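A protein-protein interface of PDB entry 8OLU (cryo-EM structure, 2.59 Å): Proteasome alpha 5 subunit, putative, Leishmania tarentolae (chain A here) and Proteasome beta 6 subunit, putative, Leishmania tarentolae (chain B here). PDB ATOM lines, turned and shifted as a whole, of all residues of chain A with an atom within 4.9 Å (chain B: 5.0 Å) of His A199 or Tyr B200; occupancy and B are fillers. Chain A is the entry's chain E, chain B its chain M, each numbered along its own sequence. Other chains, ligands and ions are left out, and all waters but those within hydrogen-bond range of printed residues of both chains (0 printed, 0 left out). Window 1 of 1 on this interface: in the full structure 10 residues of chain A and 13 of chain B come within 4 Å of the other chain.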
ATOM      1  N   GLU A 195       5.526 -10.572   5.370  1.00  0.00           N
ATOM      2  CA  GLU A 195       4.188 -10.906   5.790  1.00  0.00           C
ATOM      3  C   GLU A 195       3.387 -11.408   4.625  1.00  0.00           C
ATOM      4  O   GLU A 195       2.649 -12.373   4.776  1.00  0.00           O
ATOM      5  CB  GLU A 195       3.505  -9.739   6.484  1.00  0.00           C
ATOM      6  CG  GLU A 195       4.174  -9.447   7.847  1.00  0.00           C
ATOM      7  CD  GLU A 195       4.281 -10.601   8.868  1.00  0.00           C
ATOM      8  OE1 GLU A 195       3.430 -10.653   9.811  1.00  0.00           O
ATOM      9  OE2 GLU A 195       5.203 -11.460   8.750  1.00  0.00           O
ATOM     10  N   SER A 196       3.558 -10.838   3.457  1.00  0.00           N
ATOM     11  CA  SER A 196       2.703 -11.309   2.409  1.00  0.00           C
ATOM     12  C   SER A 196       3.068 -12.721   2.127  1.00  0.00           C
ATOM     13  O   SER A 196       2.203 -13.479   1.815  1.00  0.00           O
ATOM     14  CB  SER A 196       2.632 -10.453   1.192  1.00  0.00           C
ATOM     15  OG  SER A 196       3.883 -10.010   0.775  1.00  0.00           O
ATOM     16  N   GLN A 197       4.331 -13.069   2.227  1.00  0.00           N
ATOM     17  CA  GLN A 197       4.770 -14.399   1.893  1.00  0.00           C
ATOM     18  C   GLN A 197       4.422 -15.392   2.974  1.00  0.00           C
ATOM     19  O   GLN A 197       4.198 -16.541   2.647  1.00  0.00           O
ATOM     20  CB  GLN A 197       6.278 -14.444   1.734  1.00  0.00           C
ATOM     21  CG  GLN A 197       6.765 -14.104   0.331  1.00  0.00           C
ATOM     22  CD  GLN A 197       5.911 -14.545  -0.845  1.00  0.00           C
ATOM     23  OE1 GLN A 197       5.902 -15.709  -1.256  1.00  0.00           O
ATOM     24  NE2 GLN A 197       5.220 -13.569  -1.421  1.00  0.00           N
ATOM     25  N   ASN A 198       4.449 -14.979   4.237  1.00  0.00           N
ATOM     26  CA  ASN A 198       4.004 -15.833   5.316  1.00  0.00           C
ATOM     27  C   ASN A 198       2.537 -16.154   5.092  1.00  0.00           C
ATOM     28  O   ASN A 198       2.127 -17.302   5.241  1.00  0.00           O
ATOM     29  CB  ASN A 198       4.182 -15.240   6.714  1.00  0.00           C
ATOM     30  CG  ASN A 198       5.599 -15.326   7.258  1.00  0.00           C
ATOM     31  OD1 ASN A 198       6.312 -16.293   7.009  1.00  0.00           O
ATOM     32  ND2 ASN A 198       6.045 -14.294   7.974  1.00  0.00           N
ATOM     33  N   HIS A 199       1.749 -15.168   4.714  1.00  0.00           N
ATOM     34  CA  HIS A 199       0.382 -15.479   4.360  1.00  0.00           C
ATOM     35  C   HIS A 199       0.289 -16.512   3.261  1.00  0.00           C
ATOM     36  O   HIS A 199      -0.470 -17.433   3.381  1.00  0.00           O
ATOM     37  CB  HIS A 199      -0.361 -14.241   3.913  1.00  0.00           C
ATOM     38  CG  HIS A 199      -1.836 -14.366   3.921  1.00  0.00           C
ATOM     39  ND1 HIS A 199      -2.606 -13.951   4.968  1.00  0.00           N
ATOM     40  CD2 HIS A 199      -2.663 -14.834   2.948  1.00  0.00           C
ATOM     41  CE1 HIS A 199      -3.897 -14.152   4.642  1.00  0.00           C
ATOM     42  NE2 HIS A 199      -3.957 -14.704   3.386  1.00  0.00           N
ATOM     43  N   ARG A 200       1.013 -16.408   2.163  1.00  0.00           N
ATOM     44  CA  ARG A 200       0.867 -17.483   1.194  1.00  0.00           C
ATOM     45  C   ARG A 200       1.259 -18.800   1.792  1.00  0.00           C
ATOM     46  O   ARG A 200       0.710 -19.821   1.438  1.00  0.00           O
ATOM     47  CB  ARG A 200       1.788 -17.420   0.005  1.00  0.00           C
ATOM     48  CG  ARG A 200       1.495 -16.195  -0.821  1.00  0.00           C
ATOM     49  CD  ARG A 200       1.786 -16.605  -2.231  1.00  0.00           C
ATOM     50  NE  ARG A 200       1.624 -15.406  -3.016  1.00  0.00           N
ATOM     51  CZ  ARG A 200       0.703 -15.332  -3.945  1.00  0.00           C
ATOM     52  NH1 ARG A 200      -0.014 -16.433  -4.172  1.00  0.00           N
ATOM     53  NH2 ARG A 200       0.505 -14.166  -4.569  1.00  0.00           N
ATOM     54  N   PHE A 201       2.265 -18.749   2.640  1.00  0.00           N
ATOM     55  CA  PHE A 201       2.814 -19.985   3.104  1.00  0.00           C
ATOM     56  C   PHE A 201       1.757 -20.747   3.873  1.00  0.00           C
ATOM     57  O   PHE A 201       1.512 -21.923   3.656  1.00  0.00           O
ATOM     58  CB  PHE A 201       3.927 -19.660   4.048  1.00  0.00           C
ATOM     59  CG  PHE A 201       4.503 -20.894   4.628  1.00  0.00           C
ATOM     60  CD1 PHE A 201       5.341 -21.678   3.870  1.00  0.00           C
ATOM     61  CD2 PHE A 201       4.163 -21.303   5.883  1.00  0.00           C
ATOM     62  CE1 PHE A 201       5.840 -22.878   4.363  1.00  0.00           C
ATOM     63  CE2 PHE A 201       4.705 -22.468   6.389  1.00  0.00           C
ATOM     64  CZ  PHE A 201       5.530 -23.262   5.627  1.00  0.00           C
ATOM     65  N   THR A 202       1.122 -19.978   4.750  1.00  0.00           N
ATOM     66  CA  THR A 202       0.229 -20.442   5.773  1.00  0.00           C
ATOM     67  C   THR A 202      -1.120 -20.675   5.148  1.00  0.00           C
ATOM     68  O   THR A 202      -1.650 -21.745   5.319  1.00  0.00           O
ATOM     69  CB  THR A 202       0.201 -19.414   6.891  1.00  0.00           C
ATOM     70  OG1 THR A 202       1.221 -19.720   7.835  1.00  0.00           O
ATOM     71  CG2 THR A 202      -1.128 -19.434   7.579  1.00  0.00           C
ATOM     72  N   TYR A 203      -1.632 -19.793   4.331  1.00  0.00           N
ATOM     73  CA  TYR A 203      -2.947 -20.035   3.799  1.00  0.00           C
ATOM     74  C   TYR A 203      -2.981 -20.348   2.316  1.00  0.00           C
ATOM     75  O   TYR A 203      -4.010 -20.264   1.694  1.00  0.00           O
ATOM     76  CB  TYR A 203      -3.781 -18.780   3.993  1.00  0.00           C
ATOM     77  CG  TYR A 203      -3.842 -18.378   5.436  1.00  0.00           C
ATOM     78  CD1 TYR A 203      -4.624 -19.064   6.329  1.00  0.00           C
ATOM     79  CD2 TYR A 203      -3.191 -17.259   5.897  1.00  0.00           C
ATOM     80  CE1 TYR A 203      -4.741 -18.668   7.652  1.00  0.00           C
ATOM     81  CE2 TYR A 203      -3.240 -16.883   7.221  1.00  0.00           C
ATOM     82  CZ  TYR A 203      -3.993 -17.607   8.119  1.00  0.00           C
ATOM     83  OH  TYR A 203      -4.019 -17.207   9.455  1.00  0.00           O
ATOM     84  N   ASN A 204      -1.857 -20.525   1.674  1.00  0.00           N
ATOM     85  CA  ASN A 204      -1.824 -20.913   0.272  1.00  0.00           C
ATOM     86  C   ASN A 204      -2.671 -20.012  -0.589  1.00  0.00           C
ATOM     87  O   ASN A 204      -3.284 -20.464  -1.533  1.00  0.00           O
ATOM     88  CB  ASN A 204      -2.309 -22.339   0.110  1.00  0.00           C
ATOM     89  CG  ASN A 204      -2.065 -22.885  -1.271  1.00  0.00           C
ATOM     90  OD1 ASN A 204      -1.096 -22.482  -1.932  1.00  0.00           O
ATOM     91  ND2 ASN A 204      -2.975 -23.753  -1.700  1.00  0.00           N
ATOM     92  N   GLU A 205      -2.697 -18.732  -0.277  1.00  0.00           N
ATOM     93  CA  GLU A 205      -3.370 -17.840  -1.167  1.00  0.00           C
ATOM     94  C   GLU A 205      -2.759 -16.479  -0.996  1.00  0.00           C
ATOM     95  O   GLU A 205      -2.125 -16.240   0.000  1.00  0.00           O
ATOM     96  CB  GLU A 205      -4.839 -17.741  -0.807  1.00  0.00           C
ATOM     97  CG  GLU A 205      -5.070 -16.756   0.298  1.00  0.00           C
ATOM     98  CD  GLU A 205      -6.368 -16.824   1.060  1.00  0.00           C
ATOM     99  OE1 GLU A 205      -7.298 -17.613   0.645  1.00  0.00           O
ATOM    100  OE2 GLU A 205      -6.448 -16.037   2.056  1.00  0.00           O
ATOM    101  N   PRO A 206      -2.933 -15.576  -1.973  1.00  0.00           N
ATOM    102  CA  PRO A 206      -2.394 -14.242  -1.891  1.00  0.00           C
ATOM    103  C   PRO A 206      -3.071 -13.432  -0.801  1.00  0.00           C
ATOM    104  O   PRO A 206      -4.278 -13.428  -0.699  1.00  0.00           O
ATOM    105  CB  PRO A 206      -2.696 -13.562  -3.221  1.00  0.00           C
ATOM    106  CG  PRO A 206      -3.553 -14.514  -3.981  1.00  0.00           C
ATOM    107  CD  PRO A 206      -3.674 -15.807  -3.207  1.00  0.00           C
ATOM    108  N   MET A 207      -2.256 -12.673  -0.102  1.00  0.00           N
ATOM    109  CA  MET A 207      -2.699 -11.837   0.971  1.00  0.00           C
ATOM    110  C   MET A 207      -3.566 -10.737   0.419  1.00  0.00           C
ATOM    111  O   MET A 207      -3.248 -10.203  -0.624  1.00  0.00           O
ATOM    112  CB  MET A 207      -1.490 -11.169   1.606  1.00  0.00           C
ATOM    113  CG  MET A 207      -1.811 -10.587   2.938  1.00  0.00           C
ATOM    114  SD  MET A 207      -0.325 -10.151   3.824  1.00  0.00           S
ATOM    115  CE  MET A 207      -0.769 -10.540   5.518  1.00  0.00           C
ATOM    116  N   SER A 211      -5.067  -6.492   4.662  1.00  0.00           N
ATOM    117  CA  SER A 211      -4.272  -7.345   5.529  1.00  0.00           C
ATOM    118  C   SER A 211      -2.775  -7.064   5.456  1.00  0.00           C
ATOM    119  O   SER A 211      -2.043  -7.396   6.380  1.00  0.00           O
ATOM    120  CB  SER A 211      -4.481  -8.805   5.236  1.00  0.00           C
ATOM    121  OG  SER A 211      -3.951  -9.597   6.299  1.00  0.00           O
ATOM    122  N   TYR B 195      -9.866 -20.202  16.301  1.00  0.00           N
ATOM    123  CA  TYR B 195      -9.371 -18.881  16.604  1.00  0.00           C
ATOM    124  C   TYR B 195      -8.503 -18.332  15.484  1.00  0.00           C
ATOM    125  O   TYR B 195      -8.531 -17.140  15.229  1.00  0.00           O
ATOM    126  CB  TYR B 195      -8.725 -18.860  18.006  1.00  0.00           C
ATOM    127  CG  TYR B 195      -9.818 -18.976  19.059  1.00  0.00           C
ATOM    128  CD1 TYR B 195     -10.903 -18.082  19.025  1.00  0.00           C
ATOM    129  CD2 TYR B 195      -9.896 -20.054  19.966  1.00  0.00           C
ATOM    130  CE1 TYR B 195     -11.997 -18.226  19.872  1.00  0.00           C
ATOM    131  CE2 TYR B 195     -10.994 -20.215  20.815  1.00  0.00           C
ATOM    132  CZ  TYR B 195     -12.015 -19.256  20.802  1.00  0.00           C
ATOM    133  OH  TYR B 195     -13.133 -19.281  21.610  1.00  0.00           O
ATOM    134  N   ARG B 196      -7.710 -19.170  14.812  1.00  0.00           N
ATOM    135  CA  ARG B 196      -7.026 -18.732  13.613  1.00  0.00           C
ATOM    136  C   ARG B 196      -8.022 -18.277  12.581  1.00  0.00           C
ATOM    137  O   ARG B 196      -7.772 -17.336  11.861  1.00  0.00           O
ATOM    138  CB  ARG B 196      -6.120 -19.812  13.059  1.00  0.00           C
ATOM    139  CG  ARG B 196      -4.940 -20.109  13.972  1.00  0.00           C
ATOM    140  CD  ARG B 196      -3.980 -18.972  14.181  1.00  0.00           C
ATOM    141  NE  ARG B 196      -3.377 -18.694  12.868  1.00  0.00           N
ATOM    142  CZ  ARG B 196      -2.255 -19.262  12.387  1.00  0.00           C
ATOM    143  NH1 ARG B 196      -1.744 -18.847  11.235  1.00  0.00           N
ATOM    144  NH2 ARG B 196      -1.661 -20.226  13.090  1.00  0.00           N
ATOM    145  N   VAL B 197      -9.176 -18.868  12.541  1.00  0.00           N
ATOM    146  CA  VAL B 197     -10.157 -18.455  11.592  1.00  0.00           C
ATOM    147  C   VAL B 197     -10.772 -17.154  12.049  1.00  0.00           C
ATOM    148  O   VAL B 197     -11.063 -16.324  11.219  1.00  0.00           O
ATOM    149  CB  VAL B 197     -11.187 -19.563  11.401  1.00  0.00           C
ATOM    150  CG1 VAL B 197     -12.401 -19.138  10.604  1.00  0.00           C
ATOM    151  CG2 VAL B 197     -10.581 -20.747  10.722  1.00  0.00           C
ATOM    152  N   LYS B 198     -11.015 -16.934  13.325  1.00  0.00           N
ATOM    153  CA  LYS B 198     -11.458 -15.614  13.758  1.00  0.00           C
ATOM    154  C   LYS B 198     -10.395 -14.560  13.473  1.00  0.00           C
ATOM    155  O   LYS B 198     -10.659 -13.536  12.913  1.00  0.00           O
ATOM    156  CB  LYS B 198     -11.847 -15.584  15.240  1.00  0.00           C
ATOM    157  CG  LYS B 198     -13.328 -15.282  15.414  1.00  0.00           C
ATOM    158  CD  LYS B 198     -13.830 -14.827  16.772  1.00  0.00           C
ATOM    159  CE  LYS B 198     -14.344 -15.970  17.621  1.00  0.00           C
ATOM    160  NZ  LYS B 198     -14.484 -15.557  19.043  1.00  0.00           N
ATOM    161  N   TRP B 199      -9.151 -14.792  13.786  1.00  0.00           N
ATOM    162  CA  TRP B 199      -8.136 -13.829  13.419  1.00  0.00           C
ATOM    163  C   TRP B 199      -8.174 -13.550  11.948  1.00  0.00           C
ATOM    164  O   TRP B 199      -8.011 -12.443  11.524  1.00  0.00           O
ATOM    165  CB  TRP B 199      -6.732 -14.268  13.813  1.00  0.00           C
ATOM    166  CG  TRP B 199      -6.518 -14.030  15.261  1.00  0.00           C
ATOM    167  CD1 TRP B 199      -6.355 -14.969  16.235  1.00  0.00           C
ATOM    168  CD2 TRP B 199      -6.687 -12.778  15.939  1.00  0.00           C
ATOM    169  NE1 TRP B 199      -6.322 -14.363  17.472  1.00  0.00           N
ATOM    170  CE2 TRP B 199      -6.535 -13.026  17.310  1.00  0.00           C
ATOM    171  CE3 TRP B 199      -6.952 -11.485  15.506  1.00  0.00           C
ATOM    172  CZ2 TRP B 199      -6.561 -12.023  18.251  1.00  0.00           C
ATOM    173  CZ3 TRP B 199      -7.030 -10.480  16.438  1.00  0.00           C
ATOM    174  CH2 TRP B 199      -6.795 -10.750  17.791  1.00  0.00           C
ATOM    175  N   TYR B 200      -8.328 -14.556  11.149  1.00  0.00           N
ATOM    176  CA  TYR B 200      -8.277 -14.335   9.734  1.00  0.00           C
ATOM    177  C   TYR B 200      -9.408 -13.447   9.374  1.00  0.00           C
ATOM    178  O   TYR B 200      -9.168 -12.561   8.611  1.00  0.00           O
ATOM    179  CB  TYR B 200      -8.395 -15.659   9.001  1.00  0.00           C
ATOM    180  CG  TYR B 200      -8.376 -15.563   7.515  1.00  0.00           C
ATOM    181  CD1 TYR B 200      -9.444 -15.064   6.806  1.00  0.00           C
ATOM    182  CD2 TYR B 200      -7.235 -15.929   6.824  1.00  0.00           C
ATOM    183  CE1 TYR B 200      -9.399 -14.977   5.425  1.00  0.00           C
ATOM    184  CE2 TYR B 200      -7.186 -15.866   5.447  1.00  0.00           C
ATOM    185  CZ  TYR B 200      -8.268 -15.381   4.759  1.00  0.00           C
ATOM    186  OH  TYR B 200      -8.140 -15.369   3.415  1.00  0.00           O
ATOM    187  N   LYS B 201     -10.596 -13.696   9.903  1.00  0.00           N
ATOM    188  CA  LYS B 201     -11.741 -12.865   9.577  1.00  0.00           C
ATOM    189  C   LYS B 201     -11.421 -11.436   9.905  1.00  0.00           C
ATOM    190  O   LYS B 201     -11.681 -10.580   9.088  1.00  0.00           O
ATOM    191  CB  LYS B 201     -13.006 -13.173  10.350  1.00  0.00           C
ATOM    192  CG  LYS B 201     -13.959 -14.208   9.729  1.00  0.00           C
ATOM    193  CD  LYS B 201     -15.391 -14.258  10.384  1.00  0.00           C
ATOM    194  CE  LYS B 201     -15.879 -12.933  10.987  1.00  0.00           C
ATOM    195  NZ  LYS B 201     -15.223 -12.547  12.282  1.00  0.00           N
ATOM    196  N   TYR B 202     -10.803 -11.174  11.055  1.00  0.00           N
ATOM    197  CA  TYR B 202     -10.650  -9.790  11.484  1.00  0.00           C
ATOM    198  C   TYR B 202      -9.593  -9.084  10.648  1.00  0.00           C
ATOM    199  O   TYR B 202      -9.803  -8.000  10.157  1.00  0.00           O
ATOM    200  CB  TYR B 202     -10.213  -9.675  12.943  1.00  0.00           C
ATOM    201  CG  TYR B 202     -11.213 -10.128  13.978  1.00  0.00           C
ATOM    202  CD1 TYR B 202     -12.548  -9.838  13.835  1.00  0.00           C
ATOM    203  CD2 TYR B 202     -10.804 -10.813  15.128  1.00  0.00           C
ATOM    204  CE1 TYR B 202     -13.477 -10.234  14.794  1.00  0.00           C
ATOM    205  CE2 TYR B 202     -11.706 -11.230  16.093  1.00  0.00           C
ATOM    206  CZ  TYR B 202     -13.054 -10.941  15.914  1.00  0.00           C
ATOM    207  OH  TYR B 202     -14.031 -11.301  16.818  1.00  0.00           O
ATOM    208  N   ASN B 203      -8.462  -9.738  10.472  1.00  0.00           N
ATOM    209  CA  ASN B 203      -7.379  -9.266   9.625  1.00  0.00           C
ATOM    210  C   ASN B 203      -7.723  -9.202   8.133  1.00  0.00           C
ATOM    211  O   ASN B 203      -6.855  -8.808   7.376  1.00  0.00           O
ATOM    212  CB  ASN B 203      -6.157 -10.170   9.817  1.00  0.00           C
ATOM    213  CG  ASN B 203      -5.722 -10.137  11.255  1.00  0.00           C
ATOM    214  OD1 ASN B 203      -6.006  -9.148  11.923  1.00  0.00           O
ATOM    215  ND2 ASN B 203      -5.097 -11.193  11.761  1.00  0.00           N
ATOM    216  N   ASN B 204      -8.898  -9.669   7.675  1.00  0.00           N
ATOM    217  CA  ASN B 204      -9.227  -9.629   6.254  1.00  0.00           C
ATOM    218  C   ASN B 204     -10.631  -9.066   6.111  1.00  0.00           C
ATOM    219  O   ASN B 204     -11.446  -9.539   5.350  1.00  0.00           O
ATOM    220  CB  ASN B 204      -9.037 -10.970   5.572  1.00  0.00           C
ATOM    221  CG  ASN B 204      -7.622 -11.494   5.660  1.00  0.00           C
ATOM    222  OD1 ASN B 204      -6.834 -11.298   4.733  1.00  0.00           O
ATOM    223  ND2 ASN B 204      -7.259 -12.169   6.742  1.00  0.00           N
ATOM    224  N   LYS B 207     -13.892 -11.383   5.808  1.00  0.00           N
ATOM    225  CA  LYS B 207     -14.164 -12.516   4.946  1.00  0.00           C
ATOM    226  C   LYS B 207     -13.656 -13.803   5.583  1.00  0.00           C
ATOM    227  O   LYS B 207     -12.684 -13.847   6.317  1.00  0.00           O
ATOM    228  CB  LYS B 207     -13.644 -12.405   3.508  1.00  0.00           C
ATOM    229  CG  LYS B 207     -12.133 -12.326   3.368  1.00  0.00           C
ATOM    230  CD  LYS B 207     -11.560 -12.924   2.083  1.00  0.00           C
ATOM    231  CE  LYS B 207     -10.108 -12.518   1.895  1.00  0.00           C
ATOM    232  NZ  LYS B 207      -9.307 -13.588   1.250  1.00  0.00           N
ATOM    233  N   VAL B 208     -14.319 -14.893   5.215  1.00  0.00           N
ATOM    234  CA  VAL B 208     -13.930 -16.145   5.797  1.00  0.00           C
ATOM    235  C   VAL B 208     -12.919 -16.780   4.878  1.00  0.00           C
ATOM    236  O   VAL B 208     -13.003 -16.723   3.662  1.00  0.00           O
ATOM    237  CB  VAL B 208     -15.140 -17.056   6.051  1.00  0.00           C
ATOM    238  CG1 VAL B 208     -16.288 -16.255   6.637  1.00  0.00           C
ATOM    239  CG2 VAL B 208     -15.590 -17.748   4.783  1.00  0.00           C
ATOM    240  N   PRO B 209     -12.002 -17.507   5.474  1.00  0.00           N
ATOM    241  CA  PRO B 209     -11.010 -18.193   4.707  1.00  0.00           C
ATOM    242  C   PRO B 209     -11.679 -19.325   3.963  1.00  0.00           C
ATOM    243  O   PRO B 209     -12.666 -19.872   4.393  1.00  0.00           O
ATOM    244  CB  PRO B 209      -9.989 -18.582   5.765  1.00  0.00           C
ATOM    245  CG  PRO B 209     -10.811 -18.785   7.023  1.00  0.00           C
ATOM    246  CD  PRO B 209     -11.919 -17.762   6.906  1.00  0.00           C
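Among the printed residues, pairs that only touch across the chains: Ser A211 with Asn B204 (3.5 Å), Thr A202 with Arg B196 (3.8 Å), His A199 with Tyr B200 (3.8 Å) and Tyr A203 with Tyr B200 (3.8 Å).
The backbone carbonyl oxygen (O) of Asn B203 sits close to the side-chain hydroxyl (OG) of Ser A211. The side-chain carboxylate of Glu A205 is in salt-bridge range of the side-chain amino group of Lys B207. OH of Tyr A203 sits at hydrogen-bond distance from NH1 of Arg B196, 3.3 Å away. The side-chain hydroxyl (OH) of Tyr B200 lies close to the side-chain carboxylate (OE2) of Glu A205.
The side-chain hydroxyl of Tyr B200 sits at hydrogen-bond distance from the side-chain amino group of Lys B207 (3.0 Å). O of Trp B199 is in hydrogen-bond range of ND2 of Asn B203 (3.2 Å). O of Tyr B200 lies within hydrogen-bond range of ND2 of Asn B204, at 2.7 Å. The side-chain carboxylate of Glu A205 is in hydrogen-bond range of a ring nitrogen (NE2) of His A199, 3.1 Å away.
Hydrophobic or aromatic side chains of chain A within 4 Å of the printed part of chain B: His A199 and Tyr A203. Hydrophobic or aromatic side chains of chain B within 4 Å of the printed part of chain A: Tyr B200. Among the printed residues, Asp or Glu carboxylates within 4 Å of a Lys or Arg side-chain nitrogen of the other chain: Glu A205 with Lys B207.
Glu A195 touches none of the printed residues of chain B. Of the printed residues of chain B, His A199 touches Tyr B200. Of the printed residues of chain B, Thr A202 touches Arg B196 (3.8 Å). Of the printed residues of chain B, Glu A205 touches Tyr B200 and Lys B207. Of the printed residues of chain B, Ser A211 touches Asn B203 (3.2 Å) and Asn B204 (3.5 Å). Of the printed residues of chain A, Arg B196 touches Thr A202 (3.8 Å) and Tyr A203 (3.3 Å). Tyr B200 touches just these residues of chain A: His A199 (3.8 Å), Tyr A203 (3.8 Å) and Glu A205 (2.3 Å). Printed residues of chain A within 4 Å of Lys B207: Glu A205 (3.8 Å). The nearest residue of chain B that does not touch His A199 is Asn B204 (4.1 Å). The nearest printed residue of chain A that does not touch Tyr B200 is Pro A206 (6.0 Å).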
